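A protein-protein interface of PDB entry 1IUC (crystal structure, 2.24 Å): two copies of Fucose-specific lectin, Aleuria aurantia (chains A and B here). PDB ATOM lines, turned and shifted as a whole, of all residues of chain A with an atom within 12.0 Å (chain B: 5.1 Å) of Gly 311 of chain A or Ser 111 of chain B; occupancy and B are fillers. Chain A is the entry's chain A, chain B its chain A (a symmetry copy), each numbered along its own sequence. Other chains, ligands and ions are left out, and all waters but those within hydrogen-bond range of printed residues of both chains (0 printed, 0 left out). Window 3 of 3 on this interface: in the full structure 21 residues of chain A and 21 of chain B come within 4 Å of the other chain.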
ATOM      1  N   PRO A   1      17.775  -2.378 -19.856  1.00  0.00           N
ATOM      2  CA  PRO A   1      17.239  -2.167 -21.222  1.00  0.00           C
ATOM      3  C   PRO A   1      18.340  -2.153 -22.288  1.00  0.00           C
ATOM      4  O   PRO A   1      19.523  -2.250 -21.972  1.00  0.00           O
ATOM      5  CB  PRO A   1      16.472  -0.850 -21.201  1.00  0.00           C
ATOM      6  CG  PRO A   1      17.082  -0.150 -19.987  1.00  0.00           C
ATOM      7  CD  PRO A   1      17.363  -1.263 -18.983  1.00  0.00           C
ATOM      8  N   THR A   2      17.942  -2.035 -23.552  1.00  0.00           N
ATOM      9  CA  THR A   2      18.894  -2.037 -24.656  1.00  0.00           C
ATOM     10  C   THR A   2      18.523  -0.947 -25.650  1.00  0.00           C
ATOM     11  O   THR A   2      17.577  -0.191 -25.432  1.00  0.00           O
ATOM     12  CB  THR A   2      18.865  -3.386 -25.407  1.00  0.00           C
ATOM     13  OG1 THR A   2      17.651  -3.475 -26.168  1.00  0.00           O
ATOM     14  CG2 THR A   2      18.910  -4.553 -24.427  1.00  0.00           C
ATOM     15  N   GLU A   3      19.245  -0.893 -26.766  1.00  0.00           N
ATOM     16  CA  GLU A   3      18.970   0.116 -27.779  1.00  0.00           C
ATOM     17  C   GLU A   3      18.221  -0.464 -28.969  1.00  0.00           C
ATOM     18  O   GLU A   3      18.081   0.188 -30.003  1.00  0.00           O
ATOM     19  CB  GLU A   3      20.283   0.761 -28.216  1.00  0.00           C
ATOM     20  CG  GLU A   3      21.009   1.381 -27.043  1.00  0.00           C
ATOM     21  CD  GLU A   3      22.328   2.016 -27.424  1.00  0.00           C
ATOM     22  OE1 GLU A   3      23.196   1.326 -28.007  1.00  0.00           O
ATOM     23  OE2 GLU A   3      22.499   3.213 -27.122  1.00  0.00           O
ATOM     24  N   LEU A  30      17.048   2.675 -31.447  1.00  0.00           N
ATOM     25  CA  LEU A  30      16.117   3.738 -31.057  1.00  0.00           C
ATOM     26  C   LEU A  30      16.234   5.013 -31.904  1.00  0.00           C
ATOM     27  O   LEU A  30      15.295   5.814 -31.961  1.00  0.00           O
ATOM     28  CB  LEU A  30      16.324   4.076 -29.579  1.00  0.00           C
ATOM     29  CG  LEU A  30      16.147   2.915 -28.591  1.00  0.00           C
ATOM     30  CD1 LEU A  30      16.436   3.394 -27.187  1.00  0.00           C
ATOM     31  CD2 LEU A  30      14.722   2.372 -28.659  1.00  0.00           C
ATOM     32  N   GLY A 284      13.449  -7.491 -22.917  1.00  0.00           N
ATOM     33  CA  GLY A 284      14.838  -7.074 -22.776  1.00  0.00           C
ATOM     34  C   GLY A 284      15.075  -5.582 -22.968  1.00  0.00           C
ATOM     35  O   GLY A 284      15.549  -4.928 -22.043  1.00  0.00           O
ATOM     36  N   GLY A 307      23.257  -3.345 -27.728  1.00  0.00           N
ATOM     37  CA  GLY A 307      23.587  -2.094 -27.070  1.00  0.00           C
ATOM     38  C   GLY A 307      23.015  -1.863 -25.683  1.00  0.00           C
ATOM     39  O   GLY A 307      22.117  -2.576 -25.231  1.00  0.00           O
ATOM     40  N   THR A 308      23.556  -0.854 -25.008  1.00  0.00           N
ATOM     41  CA  THR A 308      23.126  -0.469 -23.672  1.00  0.00           C
ATOM     42  C   THR A 308      23.084   1.056 -23.658  1.00  0.00           C
ATOM     43  O   THR A 308      24.091   1.711 -23.905  1.00  0.00           O
ATOM     44  CB  THR A 308      24.129  -0.946 -22.595  1.00  0.00           C
ATOM     45  OG1 THR A 308      24.213  -2.378 -22.619  1.00  0.00           O
ATOM     46  CG2 THR A 308      23.686  -0.491 -21.207  1.00  0.00           C
ATOM     47  N   PRO A 309      21.913   1.645 -23.381  1.00  0.00           N
ATOM     48  CA  PRO A 309      21.859   3.111 -23.367  1.00  0.00           C
ATOM     49  C   PRO A 309      22.632   3.735 -22.206  1.00  0.00           C
ATOM     50  O   PRO A 309      22.909   3.082 -21.197  1.00  0.00           O
ATOM     51  CB  PRO A 309      20.361   3.403 -23.317  1.00  0.00           C
ATOM     52  CG  PRO A 309      19.810   2.234 -22.568  1.00  0.00           C
ATOM     53  CD  PRO A 309      20.591   1.052 -23.104  1.00  0.00           C
ATOM     54  N   ALA A 310      22.999   4.999 -22.369  1.00  0.00           N
ATOM     55  CA  ALA A 310      23.742   5.724 -21.342  1.00  0.00           C
ATOM     56  C   ALA A 310      22.888   5.844 -20.088  1.00  0.00           C
ATOM     57  O   ALA A 310      21.698   6.170 -20.169  1.00  0.00           O
ATOM     58  CB  ALA A 310      24.103   7.115 -21.849  1.00  0.00           C
ATOM     59  N   GLY A 311      23.506   5.589 -18.940  1.00  0.00           N
ATOM     60  CA  GLY A 311      22.812   5.677 -17.669  1.00  0.00           C
ATOM     61  C   GLY A 311      22.453   4.304 -17.150  1.00  0.00           C
ATOM     62  O   GLY A 311      21.844   4.170 -16.093  1.00  0.00           O
ATOM     63  N   TRP A 312      22.834   3.278 -17.906  1.00  0.00           N
ATOM     64  CA  TRP A 312      22.547   1.901 -17.533  1.00  0.00           C
ATOM     65  C   TRP A 312      23.792   1.029 -17.575  1.00  0.00           C
ATOM     66  O   TRP A 312      23.711  -0.110 -17.077  1.00  0.00           O
ATOM     67  CB  TRP A 312      21.491   1.318 -18.463  1.00  0.00           C
ATOM     68  CG  TRP A 312      20.177   1.997 -18.341  1.00  0.00           C
ATOM     69  CD1 TRP A 312      19.737   3.079 -19.047  1.00  0.00           C
ATOM     70  CD2 TRP A 312      19.121   1.642 -17.447  1.00  0.00           C
ATOM     71  NE1 TRP A 312      18.464   3.415 -18.649  1.00  0.00           N
ATOM     72  CE2 TRP A 312      18.065   2.547 -17.666  1.00  0.00           C
ATOM     73  CE3 TRP A 312      18.965   0.638 -16.478  1.00  0.00           C
ATOM     74  CZ2 TRP A 312      16.866   2.485 -16.954  1.00  0.00           C
ATOM     75  CZ3 TRP A 312      17.772   0.575 -15.770  1.00  0.00           C
ATOM     76  CH2 TRP A 312      16.739   1.494 -16.013  1.00  0.00           C
ATOM     77  OXT TRP A 312      24.816   1.485 -18.121  1.00  0.00           O
ATOM     78  N   LYS B  58      17.597  10.533 -19.212  1.00  0.00           N
ATOM     79  CA  LYS B  58      18.215   9.344 -19.773  1.00  0.00           C
ATOM     80  C   LYS B  58      17.077   8.481 -20.330  1.00  0.00           C
ATOM     81  O   LYS B  58      15.916   8.654 -19.943  1.00  0.00           O
ATOM     82  CB  LYS B  58      18.975   8.577 -18.688  1.00  0.00           C
ATOM     83  CG  LYS B  58      18.088   7.810 -17.700  1.00  0.00           C
ATOM     84  CD  LYS B  58      18.946   6.983 -16.760  1.00  0.00           C
ATOM     85  CE  LYS B  58      18.137   5.977 -15.954  1.00  0.00           C
ATOM     86  NZ  LYS B  58      19.056   5.058 -15.197  1.00  0.00           N
ATOM     87  N   LYS B  83      21.546  11.221 -17.751  1.00  0.00           N
ATOM     88  CA  LYS B  83      22.420  10.133 -18.161  1.00  0.00           C
ATOM     89  C   LYS B  83      23.480   9.751 -17.149  1.00  0.00           C
ATOM     90  O   LYS B  83      24.142   8.726 -17.300  1.00  0.00           O
ATOM     91  CB  LYS B  83      23.059  10.452 -19.509  1.00  0.00           C
ATOM     92  CG  LYS B  83      22.040  10.603 -20.620  1.00  0.00           C
ATOM     93  CD  LYS B  83      22.705  10.800 -21.962  1.00  0.00           C
ATOM     94  CE  LYS B  83      21.667  11.082 -23.034  1.00  0.00           C
ATOM     95  NZ  LYS B  83      22.286  11.342 -24.378  1.00  0.00           N
ATOM     96  N   ASN B  85      22.590   9.534 -13.958  1.00  0.00           N
ATOM     97  CA  ASN B  85      21.732   9.091 -12.856  1.00  0.00           C
ATOM     98  C   ASN B  85      21.614  10.108 -11.724  1.00  0.00           C
ATOM     99  O   ASN B  85      21.554   9.756 -10.543  1.00  0.00           O
ATOM    100  CB  ASN B  85      22.204   7.731 -12.312  1.00  0.00           C
ATOM    101  CG  ASN B  85      21.871   6.587 -13.262  1.00  0.00           C
ATOM    102  OD1 ASN B  85      20.721   6.435 -13.683  1.00  0.00           O
ATOM    103  ND2 ASN B  85      22.871   5.778 -13.601  1.00  0.00           N
ATOM    104  N   VAL B 109      21.052   8.426  -8.080  1.00  0.00           N
ATOM    105  CA  VAL B 109      20.011   7.406  -7.999  1.00  0.00           C
ATOM    106  C   VAL B 109      20.487   6.083  -8.603  1.00  0.00           C
ATOM    107  O   VAL B 109      21.331   6.072  -9.498  1.00  0.00           O
ATOM    108  CB  VAL B 109      18.748   7.886  -8.759  1.00  0.00           C
ATOM    109  CG1 VAL B 109      17.693   6.806  -8.766  1.00  0.00           C
ATOM    110  CG2 VAL B 109      18.205   9.155  -8.104  1.00  0.00           C
ATOM    111  N   GLY B 110      19.964   4.971  -8.091  1.00  0.00           N
ATOM    112  CA  GLY B 110      20.330   3.676  -8.634  1.00  0.00           C
ATOM    113  C   GLY B 110      19.791   3.662 -10.051  1.00  0.00           C
ATOM    114  O   GLY B 110      18.705   4.197 -10.298  1.00  0.00           O
ATOM    115  N   SER B 111      20.526   3.058 -10.983  1.00  0.00           N
ATOM    116  CA  SER B 111      20.090   3.035 -12.380  1.00  0.00           C
ATOM    117  C   SER B 111      18.699   2.464 -12.612  1.00  0.00           C
ATOM    118  O   SER B 111      17.979   2.950 -13.488  1.00  0.00           O
ATOM    119  CB  SER B 111      21.106   2.284 -13.258  1.00  0.00           C
ATOM    120  OG  SER B 111      21.388   1.001 -12.733  1.00  0.00           O
ATOM    121  N   ASN B 112      18.311   1.461 -11.825  1.00  0.00           N
ATOM    122  CA  ASN B 112      16.997   0.831 -11.984  1.00  0.00           C
ATOM    123  C   ASN B 112      15.947   1.327 -10.993  1.00  0.00           C
ATOM    124  O   ASN B 112      14.894   0.712 -10.840  1.00  0.00           O
ATOM    125  CB  ASN B 112      17.120  -0.695 -11.859  1.00  0.00           C
ATOM    126  CG  ASN B 112      15.890  -1.427 -12.396  1.00  0.00           C
ATOM    127  OD1 ASN B 112      15.380  -1.109 -13.479  1.00  0.00           O
ATOM    128  ND2 ASN B 112      15.416  -2.414 -11.649  1.00  0.00           N
ATOM    129  N   SER B 113      16.228   2.444 -10.326  1.00  0.00           N
ATOM    130  CA  SER B 113      15.293   2.986  -9.350  1.00  0.00           C
ATOM    131  C   SER B 113      14.068   3.628  -9.985  1.00  0.00           C
ATOM    132  O   SER B 113      14.121   4.131 -11.109  1.00  0.00           O
ATOM    133  CB  SER B 113      16.009   4.020  -8.473  1.00  0.00           C
ATOM    134  OG  SER B 113      15.099   4.759  -7.680  1.00  0.00           O
ATOM    135  N   ASN B 138      20.347  -0.863  -6.665  1.00  0.00           N
ATOM    136  CA  ASN B 138      19.426  -1.756  -7.359  1.00  0.00           C
ATOM    137  C   ASN B 138      19.353  -3.135  -6.713  1.00  0.00           C
ATOM    138  O   ASN B 138      18.587  -3.991  -7.157  1.00  0.00           O
ATOM    139  CB  ASN B 138      19.853  -1.909  -8.825  1.00  0.00           C
ATOM    140  CG  ASN B 138      20.066  -0.572  -9.514  1.00  0.00           C
ATOM    141  OD1 ASN B 138      19.168   0.274  -9.549  1.00  0.00           O
ATOM    142  ND2 ASN B 138      21.257  -0.376 -10.069  1.00  0.00           N
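The side-chain amino group (NZ) of Lys 58 of chain B sits at hydrogen-bond distance from the side-chain amide oxygen (OD1) of Asn 85 of chain B.
The side-chain amino group (NZ) of Lys 58 of chain B lies within hydrogen-bond range of the backbone carbonyl oxygen (O) of Ser 111 of chain B.
The backbone NH of Val 109 of chain B sits at hydrogen-bond distance from the backbone carbonyl oxygen of Asn 85 of chain B (2.8 Å).
OG of Ser 111 of chain B is in hydrogen-bond range of ND2 of Asn 138 of chain B, at 3.0 Å.
N of Asn 112 of chain B is in hydrogen-bond range of OD1 of Asn 138 of chain B (2.7 Å).
Glu 3 of chain A touches none of the printed residues of chain B.
Of the printed residues of chain B, Ala 310 of chain A touches Lys 58 (3.9 Å) and Lys 83 (3.9 Å).
Gly 311 of chain A touches four residues of chain B.
Of the printed residues of chain B, Trp 312 of chain A touches Lys 58 (3.7 Å), Ser 111 (3.2 Å) and Asn 112 (3.7 Å).
Lys 58 of chain B touches just these residues of chain A: Ala 310, Gly 311 and Trp 312.
Of the printed residues of chain A, Lys 83 of chain B touches Ala 310 (3.9 Å) and Gly 311 (3.3 Å).
Asn 85 of chain B touches one residue of chain A.
No residue of chain A comes within 4 Å of Val 109 of chain B.
Ser 111 of chain B touches two residues of chain A.
Asn 112 of chain B touches one residue of chain A.
No residue of chain A comes within 4 Å of Ser 113 of chain B.
The nearest printed residue of chain B that does not touch Ala 310 of chain A is Asn 85 of chain B (6.5 Å).
The backbone carbonyl oxygen of Gly 311 of chain A is in hydrogen-bond range of the side-chain amino group of Lys 58 of chain B (3.1 Å).
The side-chain amide nitrogen of Asn 85 of chain B sits at hydrogen-bond distance from the backbone carbonyl oxygen of Gly 311 of chain A (3.1 Å).
Lys 58 of chain B touches Ala 310 of chain A (CB to O, 3.9 Å).
Ala 310 of chain A touches Lys 83 of chain B.
Gly 311 of chain A touches Lys 83 of chain B.
O of Gly 311 of chain A touches CB of Ser 111 of chain B, 3.5 Å away.
NZ of Lys 58 of chain B touches CE2 of Trp 312 of chain A, at 3.7 Å.
Ser 111 of chain B touches Trp 312 of chain A (O to CH2, 3.2 Å).
Asn 112 of chain B touches Trp 312 of chain A (OD1 to CZ3, 3.7 Å).
No position is printed for both chains.
Hydrophobic or aromatic side chains of chain A that line the printed part of chain B: Ala 310 and Trp 312.
Among the printed residues, 9 pairs touch across the chains.
Among the printed residues, no Asp or Glu carboxylate lies within 4 Å of a Lys or Arg side-chain nitrogen of the other chain.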
